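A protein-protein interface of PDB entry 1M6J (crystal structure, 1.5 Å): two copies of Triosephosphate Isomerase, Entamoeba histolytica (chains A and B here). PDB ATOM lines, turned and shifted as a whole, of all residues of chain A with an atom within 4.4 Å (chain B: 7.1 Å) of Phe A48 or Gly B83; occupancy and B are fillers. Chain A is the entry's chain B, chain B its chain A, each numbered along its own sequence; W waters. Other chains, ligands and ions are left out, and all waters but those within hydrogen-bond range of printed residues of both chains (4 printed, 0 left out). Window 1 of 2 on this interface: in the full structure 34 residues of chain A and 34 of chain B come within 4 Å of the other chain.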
ATOM      1  N   VAL A  46      -6.466  27.457 -18.910  1.00  0.00           N
ATOM      2  CA  VAL A  46      -6.730  28.490 -19.906  1.00  0.00           C
ATOM      3  C   VAL A  46      -8.098  28.422 -20.583  1.00  0.00           C
ATOM      4  O   VAL A  46      -8.580  27.340 -20.902  1.00  0.00           O
ATOM      5  CB  VAL A  46      -5.661  28.387 -21.020  1.00  0.00           C
ATOM      6  CG1 VAL A  46      -5.778  29.552 -21.982  1.00  0.00           C
ATOM      7  CG2 VAL A  46      -4.270  28.318 -20.405  1.00  0.00           C
ATOM      8  N   PRO A  47      -8.739  29.583 -20.814  1.00  0.00           N
ATOM      9  CA  PRO A  47     -10.049  29.560 -21.480  1.00  0.00           C
ATOM     10  C   PRO A  47      -9.850  28.927 -22.864  1.00  0.00           C
ATOM     11  O   PRO A  47      -8.838  29.175 -23.515  1.00  0.00           O
ATOM     12  CB  PRO A  47     -10.416  31.038 -21.565  1.00  0.00           C
ATOM     13  CG  PRO A  47      -9.772  31.606 -20.325  1.00  0.00           C
ATOM     14  CD  PRO A  47      -8.417  30.939 -20.333  1.00  0.00           C
ATOM     15  N   PHE A  48     -10.813  28.124 -23.316  1.00  0.00           N
ATOM     16  CA  PHE A  48     -10.695  27.426 -24.600  1.00  0.00           C
ATOM     17  C   PHE A  48     -10.103  28.213 -25.764  1.00  0.00           C
ATOM     18  O   PHE A  48      -9.155  27.768 -26.406  1.00  0.00           O
ATOM     19  CB  PHE A  48     -12.054  26.902 -25.077  1.00  0.00           C
ATOM     20  CG  PHE A  48     -12.660  25.842 -24.204  1.00  0.00           C
ATOM     21  CD1 PHE A  48     -11.972  24.669 -23.912  1.00  0.00           C
ATOM     22  CD2 PHE A  48     -13.955  25.997 -23.721  1.00  0.00           C
ATOM     23  CE1 PHE A  48     -12.569  23.658 -23.150  1.00  0.00           C
ATOM     24  CE2 PHE A  48     -14.561  24.995 -22.962  1.00  0.00           C
ATOM     25  CZ  PHE A  48     -13.864  23.825 -22.678  1.00  0.00           C
ATOM     26  N   ILE A  49     -10.684  29.375 -26.041  1.00  0.00           N
ATOM     27  CA  ILE A  49     -10.265  30.192 -27.172  1.00  0.00           C
ATOM     28  C   ILE A  49      -8.823  30.681 -27.133  1.00  0.00           C
ATOM     29  O   ILE A  49      -8.245  30.995 -28.175  1.00  0.00           O
ATOM     30  CB  ILE A  49     -11.229  31.396 -27.351  1.00  0.00           C
ATOM     31  CG1 ILE A  49     -11.111  31.954 -28.771  1.00  0.00           C
ATOM     32  CG2 ILE A  49     -10.935  32.472 -26.312  1.00  0.00           C
ATOM     33  CD1 ILE A  49     -12.203  32.948 -29.122  1.00  0.00           C
ATOM     34  N   TYR A  50      -8.236  30.720 -25.942  1.00  0.00           N
ATOM     35  CA  TYR A  50      -6.860  31.182 -25.791  1.00  0.00           C
ATOM     36  C   TYR A  50      -5.827  30.065 -25.675  1.00  0.00           C
ATOM     37  O   TYR A  50      -4.634  30.333 -25.541  1.00  0.00           O
ATOM     38  CB  TYR A  50      -6.753  32.101 -24.571  1.00  0.00           C
ATOM     39  CG  TYR A  50      -7.469  33.423 -24.751  1.00  0.00           C
ATOM     40  CD1 TYR A  50      -8.482  33.812 -23.879  1.00  0.00           C
ATOM     41  CD2 TYR A  50      -7.132  34.283 -25.793  1.00  0.00           C
ATOM     42  CE1 TYR A  50      -9.144  35.027 -24.036  1.00  0.00           C
ATOM     43  CE2 TYR A  50      -7.786  35.504 -25.961  1.00  0.00           C
ATOM     44  CZ  TYR A  50      -8.791  35.868 -25.079  1.00  0.00           C
ATOM     45  OH  TYR A  50      -9.444  37.068 -25.236  1.00  0.00           O
ATOM     46  N   ILE A  51      -6.270  28.813 -25.727  1.00  0.00           N
ATOM     47  CA  ILE A  51      -5.331  27.706 -25.621  1.00  0.00           C
ATOM     48  C   ILE A  51      -4.279  27.750 -26.733  1.00  0.00           C
ATOM     49  O   ILE A  51      -3.095  27.587 -26.469  1.00  0.00           O
ATOM     50  CB  ILE A  51      -6.075  26.349 -25.598  1.00  0.00           C
ATOM     51  CG1 ILE A  51      -6.719  26.169 -24.221  1.00  0.00           C
ATOM     52  CG2 ILE A  51      -5.115  25.199 -25.902  1.00  0.00           C
ATOM     53  CD1 ILE A  51      -7.554  24.915 -24.070  1.00  0.00           C
ATOM     54  N   PRO A  52      -4.695  27.980 -27.988  1.00  0.00           N
ATOM     55  CA  PRO A  52      -3.699  28.032 -29.062  1.00  0.00           C
ATOM     56  C   PRO A  52      -2.666  29.139 -28.829  1.00  0.00           C
ATOM     57  O   PRO A  52      -1.473  28.937 -29.044  1.00  0.00           O
ATOM     58  CB  PRO A  52      -4.549  28.281 -30.306  1.00  0.00           C
ATOM     59  CG  PRO A  52      -5.809  27.544 -29.982  1.00  0.00           C
ATOM     60  CD  PRO A  52      -6.061  27.955 -28.540  1.00  0.00           C
ATOM     61  N   ALA A  71      -7.172  22.648 -19.924  1.00  0.00           N
ATOM     62  CA  ALA A  71      -8.411  23.283 -20.225  1.00  0.00           C
ATOM     63  C   ALA A  71      -9.150  23.402 -18.930  1.00  0.00           C
ATOM     64  O   ALA A  71      -8.812  22.779 -17.932  1.00  0.00           O
ATOM     65  CB  ALA A  71      -9.190  22.387 -21.190  1.00  0.00           C
ATOM     66  N   GLU A  72     -10.188  24.226 -18.877  1.00  0.00           N
ATOM     67  CA  GLU A  72     -10.930  24.440 -17.639  1.00  0.00           C
ATOM     68  C   GLU A  72     -12.192  23.594 -17.530  1.00  0.00           C
ATOM     69  O   GLU A  72     -12.896  23.649 -16.522  1.00  0.00           O
ATOM     70  CB  GLU A  72     -11.303  25.914 -17.511  1.00  0.00           C
ATOM     71  CG  GLU A  72     -10.111  26.828 -17.314  1.00  0.00           C
ATOM     72  CD  GLU A  72     -10.516  28.279 -17.200  1.00  0.00           C
ATOM     73  OE1 GLU A  72     -11.681  28.538 -16.831  1.00  0.00           O
ATOM     74  OE2 GLU A  72      -9.670  29.161 -17.469  1.00  0.00           O
ATOM     75  N   ASN A  73     -12.472  22.820 -18.572  1.00  0.00           N
ATOM     76  CA  ASN A  73     -13.651  21.965 -18.610  1.00  0.00           C
ATOM     77  C   ASN A  73     -13.612  21.181 -19.911  1.00  0.00           C
ATOM     78  O   ASN A  73     -12.765  21.431 -20.769  1.00  0.00           O
ATOM     79  CB  ASN A  73     -14.921  22.829 -18.552  1.00  0.00           C
ATOM     80  CG  ASN A  73     -16.200  22.011 -18.664  1.00  0.00           C
ATOM     81  OD1 ASN A  73     -16.346  20.979 -18.017  1.00  0.00           O
ATOM     82  ND2 ASN A  73     -17.140  22.486 -19.479  1.00  0.00           N
ATOM     83  N   VAL A  85     -16.981  21.962 -25.978  1.00  0.00           N
ATOM     84  CA  VAL A  85     -15.689  21.531 -26.495  1.00  0.00           C
ATOM     85  C   VAL A  85     -15.462  20.133 -25.923  1.00  0.00           C
ATOM     86  O   VAL A  85     -15.407  19.940 -24.707  1.00  0.00           O
ATOM     87  CB  VAL A  85     -14.555  22.486 -26.062  1.00  0.00           C
ATOM     88  CG1 VAL A  85     -13.208  21.951 -26.539  1.00  0.00           C
ATOM     89  CG2 VAL A  85     -14.796  23.870 -26.664  1.00  0.00           C
ATOM     90  N   LEU A  90      -9.546  18.451 -27.131  1.00  0.00           N
ATOM     91  CA  LEU A  90      -8.406  18.834 -26.306  1.00  0.00           C
ATOM     92  C   LEU A  90      -7.215  17.955 -26.672  1.00  0.00           C
ATOM     93  O   LEU A  90      -6.099  18.445 -26.855  1.00  0.00           O
ATOM     94  CB  LEU A  90      -8.733  18.662 -24.821  1.00  0.00           C
ATOM     95  CG  LEU A  90      -9.921  19.456 -24.277  1.00  0.00           C
ATOM     96  CD1 LEU A  90     -10.004  19.252 -22.768  1.00  0.00           C
ATOM     97  CD2 LEU A  90      -9.765  20.937 -24.611  1.00  0.00           C
ATOM     98  N   ARG A 105     -18.673  25.074 -11.765  1.00  0.00           N
ATOM     99  CA  ARG A 105     -19.456  24.326 -12.739  1.00  0.00           C
ATOM    100  C   ARG A 105     -20.481  23.437 -12.044  1.00  0.00           C
ATOM    101  O   ARG A 105     -21.581  23.229 -12.559  1.00  0.00           O
ATOM    102  CB  ARG A 105     -18.538  23.495 -13.634  1.00  0.00           C
ATOM    103  CG  ARG A 105     -17.579  24.351 -14.450  1.00  0.00           C
ATOM    104  CD  ARG A 105     -17.285  23.713 -15.793  1.00  0.00           C
ATOM    105  NE  ARG A 105     -18.489  23.658 -16.621  1.00  0.00           N
ATOM    106  CZ  ARG A 105     -18.960  24.675 -17.338  1.00  0.00           C
ATOM    107  NH1 ARG A 105     -18.334  25.846 -17.347  1.00  0.00           N
ATOM    108  NH2 ARG A 105     -20.074  24.520 -18.039  1.00  0.00           N
ATOM    109  N   PRO B  47     -16.207  25.482 -32.783  1.00  0.00           N
ATOM    110  CA  PRO B  47     -15.943  25.224 -31.361  1.00  0.00           C
ATOM    111  C   PRO B  47     -14.858  26.208 -30.909  1.00  0.00           C
ATOM    112  O   PRO B  47     -13.927  26.495 -31.663  1.00  0.00           O
ATOM    113  CB  PRO B  47     -15.459  23.773 -31.358  1.00  0.00           C
ATOM    114  CG  PRO B  47     -16.228  23.166 -32.498  1.00  0.00           C
ATOM    115  CD  PRO B  47     -16.130  24.236 -33.569  1.00  0.00           C
ATOM    116  N   PHE B  48     -14.973  26.717 -29.686  1.00  0.00           N
ATOM    117  CA  PHE B  48     -14.017  27.703 -29.174  1.00  0.00           C
ATOM    118  C   PHE B  48     -12.548  27.444 -29.482  1.00  0.00           C
ATOM    119  O   PHE B  48     -11.846  28.313 -29.999  1.00  0.00           O
ATOM    120  CB  PHE B  48     -14.129  27.843 -27.654  1.00  0.00           C
ATOM    121  CG  PHE B  48     -15.424  28.434 -27.172  1.00  0.00           C
ATOM    122  CD1 PHE B  48     -15.864  29.676 -27.628  1.00  0.00           C
ATOM    123  CD2 PHE B  48     -16.177  27.767 -26.212  1.00  0.00           C
ATOM    124  CE1 PHE B  48     -17.038  30.245 -27.126  1.00  0.00           C
ATOM    125  CE2 PHE B  48     -17.349  28.324 -25.703  1.00  0.00           C
ATOM    126  CZ  PHE B  48     -17.780  29.566 -26.161  1.00  0.00           C
ATOM    127  N   ILE B  49     -12.081  26.251 -29.137  1.00  0.00           N
ATOM    128  CA  ILE B  49     -10.676  25.907 -29.306  1.00  0.00           C
ATOM    129  C   ILE B  49     -10.168  25.900 -30.745  1.00  0.00           C
ATOM    130  O   ILE B  49      -8.961  26.007 -30.979  1.00  0.00           O
ATOM    131  CB  ILE B  49     -10.380  24.541 -28.628  1.00  0.00           C
ATOM    132  CG1 ILE B  49      -8.877  24.395 -28.373  1.00  0.00           C
ATOM    133  CG2 ILE B  49     -10.910  23.401 -29.493  1.00  0.00           C
ATOM    134  CD1 ILE B  49      -8.519  23.223 -27.468  1.00  0.00           C
ATOM    135  N   TYR B  50     -11.078  25.795 -31.709  1.00  0.00           N
ATOM    136  CA  TYR B  50     -10.675  25.772 -33.113  1.00  0.00           C
ATOM    137  C   TYR B  50     -10.848  27.109 -33.819  1.00  0.00           C
ATOM    138  O   TYR B  50     -10.537  27.230 -34.999  1.00  0.00           O
ATOM    139  CB  TYR B  50     -11.456  24.697 -33.879  1.00  0.00           C
ATOM    140  CG  TYR B  50     -11.105  23.283 -33.487  1.00  0.00           C
ATOM    141  CD1 TYR B  50     -12.085  22.407 -33.022  1.00  0.00           C
ATOM    142  CD2 TYR B  50      -9.793  22.815 -33.587  1.00  0.00           C
ATOM    143  CE1 TYR B  50     -11.771  21.100 -32.666  1.00  0.00           C
ATOM    144  CE2 TYR B  50      -9.467  21.504 -33.231  1.00  0.00           C
ATOM    145  CZ  TYR B  50     -10.463  20.655 -32.771  1.00  0.00           C
ATOM    146  OH  TYR B  50     -10.157  19.362 -32.420  1.00  0.00           O
ATOM    147  N   ILE B  51     -11.337  28.118 -33.107  1.00  0.00           N
ATOM    148  CA  ILE B  51     -11.533  29.419 -33.732  1.00  0.00           C
ATOM    149  C   ILE B  51     -10.233  29.999 -34.282  1.00  0.00           C
ATOM    150  O   ILE B  51     -10.201  30.483 -35.408  1.00  0.00           O
ATOM    151  CB  ILE B  51     -12.220  30.406 -32.755  1.00  0.00           C
ATOM    152  CG1 ILE B  51     -13.704  30.030 -32.639  1.00  0.00           C
ATOM    153  CG2 ILE B  51     -12.057  31.848 -33.246  1.00  0.00           C
ATOM    154  CD1 ILE B  51     -14.488  30.812 -31.596  1.00  0.00           C
ATOM    155  N   PRO B  52      -9.140  29.951 -33.504  1.00  0.00           N
ATOM    156  CA  PRO B  52      -7.896  30.506 -34.043  1.00  0.00           C
ATOM    157  C   PRO B  52      -7.460  29.797 -35.329  1.00  0.00           C
ATOM    158  O   PRO B  52      -7.024  30.444 -36.282  1.00  0.00           O
ATOM    159  CB  PRO B  52      -6.904  30.304 -32.898  1.00  0.00           C
ATOM    160  CG  PRO B  52      -7.777  30.440 -31.688  1.00  0.00           C
ATOM    161  CD  PRO B  52      -8.980  29.603 -32.081  1.00  0.00           C
ATOM    162  N   TYR B  81     -15.913  32.012 -13.458  1.00  0.00           N
ATOM    163  CA  TYR B  81     -16.797  31.126 -14.201  1.00  0.00           C
ATOM    164  C   TYR B  81     -15.939  30.125 -14.960  1.00  0.00           C
ATOM    165  O   TYR B  81     -15.837  30.159 -16.190  1.00  0.00           O
ATOM    166  CB  TYR B  81     -17.659  31.946 -15.159  1.00  0.00           C
ATOM    167  CG  TYR B  81     -18.369  33.080 -14.461  1.00  0.00           C
ATOM    168  CD1 TYR B  81     -17.907  34.389 -14.571  1.00  0.00           C
ATOM    169  CD2 TYR B  81     -19.474  32.835 -13.648  1.00  0.00           C
ATOM    170  CE1 TYR B  81     -18.524  35.431 -13.889  1.00  0.00           C
ATOM    171  CE2 TYR B  81     -20.101  33.871 -12.956  1.00  0.00           C
ATOM    172  CZ  TYR B  81     -19.620  35.165 -13.083  1.00  0.00           C
ATOM    173  OH  TYR B  81     -20.232  36.196 -12.405  1.00  0.00           O
ATOM    174  N   THR B  82     -15.313  29.233 -14.202  1.00  0.00           N
ATOM    175  CA  THR B  82     -14.435  28.220 -14.763  1.00  0.00           C
ATOM    176  C   THR B  82     -15.079  27.452 -15.913  1.00  0.00           C
ATOM    177  O   THR B  82     -16.192  26.940 -15.789  1.00  0.00           O
ATOM    178  CB  THR B  82     -13.977  27.243 -13.659  1.00  0.00           C
ATOM    179  OG1 THR B  82     -13.209  27.968 -12.692  1.00  0.00           O
ATOM    180  CG2 THR B  82     -13.108  26.134 -14.234  1.00  0.00           C
ATOM    181  N   GLY B  83     -14.370  27.404 -17.039  1.00  0.00           N
ATOM    182  CA  GLY B  83     -14.852  26.694 -18.211  1.00  0.00           C
ATOM    183  C   GLY B  83     -15.537  27.554 -19.255  1.00  0.00           C
ATOM    184  O   GLY B  83     -15.703  27.129 -20.396  1.00  0.00           O
ATOM    185  N   GLU B  84     -15.917  28.767 -18.878  1.00  0.00           N
ATOM    186  CA  GLU B  84     -16.621  29.669 -19.788  1.00  0.00           C
ATOM    187  C   GLU B  84     -15.743  30.616 -20.593  1.00  0.00           C
ATOM    188  O   GLU B  84     -14.636  30.960 -20.186  1.00  0.00           O
ATOM    189  CB  GLU B  84     -17.622  30.518 -18.998  1.00  0.00           C
ATOM    190  CG  GLU B  84     -18.704  29.725 -18.294  1.00  0.00           C
ATOM    191  CD  GLU B  84     -19.561  28.937 -19.261  1.00  0.00           C
ATOM    192  OE1 GLU B  84     -20.196  29.564 -20.138  1.00  0.00           O
ATOM    193  OE2 GLU B  84     -19.593  27.694 -19.144  1.00  0.00           O
ATOM    194  N   VAL B  85     -16.262  31.037 -21.745  1.00  0.00           N
ATOM    195  CA  VAL B  85     -15.625  32.009 -22.574  1.00  0.00           C
ATOM    196  C   VAL B  85     -16.583  33.152 -22.721  1.00  0.00           C
ATOM    197  O   VAL B  85     -17.691  33.007 -23.222  1.00  0.00           O
ATOM    198  CB  VAL B  85     -15.357  31.373 -23.938  1.00  0.00           C
ATOM    199  CG1 VAL B  85     -14.855  32.432 -24.918  1.00  0.00           C
ATOM    200  CG2 VAL B  85     -14.312  30.280 -23.805  1.00  0.00           C
ATOM    201  N   MET B  89     -13.961  38.077 -24.816  1.00  0.00           N
ATOM    202  CA  MET B  89     -12.863  37.302 -25.371  1.00  0.00           C
ATOM    203  C   MET B  89     -13.075  37.103 -26.865  1.00  0.00           C
ATOM    204  O   MET B  89     -12.117  37.059 -27.632  1.00  0.00           O
ATOM    205  CB  MET B  89     -12.764  35.949 -24.673  1.00  0.00           C
ATOM    206  CG  MET B  89     -12.615  36.051 -23.169  1.00  0.00           C
ATOM    207  SD  MET B  89     -12.563  34.426 -22.407  1.00  0.00           S
ATOM    208  CE  MET B  89     -11.652  34.807 -20.895  1.00  0.00           C
HETATM  209  O   HOH W   1     -12.661  29.473 -19.341  1.00  0.00           O
HETATM  210  O   HOH W   2     -21.712  26.274 -19.834  1.00  0.00           O
HETATM  211  O   HOH W   3     -17.337  24.868 -21.070  1.00  0.00           O
HETATM  212  O   HOH W   4     -12.812  27.485 -21.178  1.00  0.00           O
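Phe A48 touches three residues of chain B.
Of the printed residues of chain B, Leu A90 touches Ile B49 (3.9 Å).
Printed residues of chain A within 4 Å of Ile B49: Phe A48 (3.8 Å), Ile A51 (3.9 Å), Pro A52 (3.6 Å) and Leu A90 (3.9 Å).
Tyr B50 touches none of the printed residues of chain A.
Printed residues of chain A within 4 Å of Thr B82: Glu A72 and Arg A105.
The nearest printed residue of chain A that does not touch Gly B83 is Pro A47 (6.2 Å).
Phe B48 touches its own counterpart, Phe A48.
Phe A48 touches Ile B49, and with the chains exchanged Ile A49 touches Phe B48.
Ile A49 touches Ile B51, and with the chains exchanged Ile A51 touches Ile B49.
Pro A52 touches its own counterpart, Pro B52.
Of the 18 pairs that touch across the chains among the printed residues, 8 have their exchanged pair printed and touching as well.
O of Thr B82 sits at hydrogen-bond distance from NH1 of Arg A105 (2.9 Å).
The backbone NH (N) of Gly B83 is in hydrogen-bond range of the side-chain carboxylate (OE1) of Glu A72, at 2.9 Å.
The side-chain carboxylate (OE2) of Glu B84 is in salt-bridge range of the guanidinium group (NH1) of Arg A105 (2.9 Å).
Among the printed residues, merely in contact across the chains: Pro A47 with Met B89 (3.8 Å), Phe A48 with Phe B48 (3.4 Å), Phe A48 with Ile B49 (3.8 Å), Phe A48 with Gly B83 (3.5 Å), Ile A49 with Phe B48 (3.7 Å), Ile A49 with Ile B51 (3.99 Å), Ile A49 with Pro B52 (3.6 Å), Tyr A50 with Met B89 (3.4 Å), Ile A51 with Ile B49 (3.9 Å), Pro A52 with Ile B49 (3.6 Å), Pro A52 with Pro B52 (3.9 Å), Glu A72 with Thr B82 (3.4 Å), Asn A73 with Gly B83 (3.9 Å), Leu A90 with Ile B49 (3.9 Å) and Arg A105 with Gly B83 (3.7 Å).
Water W1 bridges O of Glu B84 (2.6 Å) and OE1 of Glu A72 (2.9 Å).
Water W2 bridges OE2 of Glu B84 (2.6 Å) and NH2 of Arg A105 (3.0 Å).
Water W3 lies within hydrogen-bond range of O of Gly B83 and ND2 of Asn A73.
Water W4 bridges N of Phe A48 (3.0 Å) and O of Gly B83 (3.0 Å).
Of the 12 printed residues of chain B, 8 touch a printed residue of chain A.
Printed residues of chain B that touch a printed residue of chain A: Phe B48, Ile B49, Ile B51, Pro B52, Thr B82, Gly B83, Glu B84 and Met B89.
Hydrophobic or aromatic side chains of chain B within 4 Å of the printed part of chain A: Phe B48, Ile B49, Ile B51, Pro B52 and Met B89.
Of the 13 printed residues of chain A, 10 touch a printed residue of chain B.
Hydrophobic or aromatic side chains of chain A that line the printed part of chain B: Pro A47, Phe A48, Ile A49, Tyr A50, Ile A51, Pro A52 and Leu A90.
Among the printed residues, Asp or Glu carboxylates within 4 Å of a Lys or Arg side-chain nitrogen of the other chain: Arg A105 with Glu B84.
NE of Arg A105 lies close to ND2 of Asn A73 (3.4 Å).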
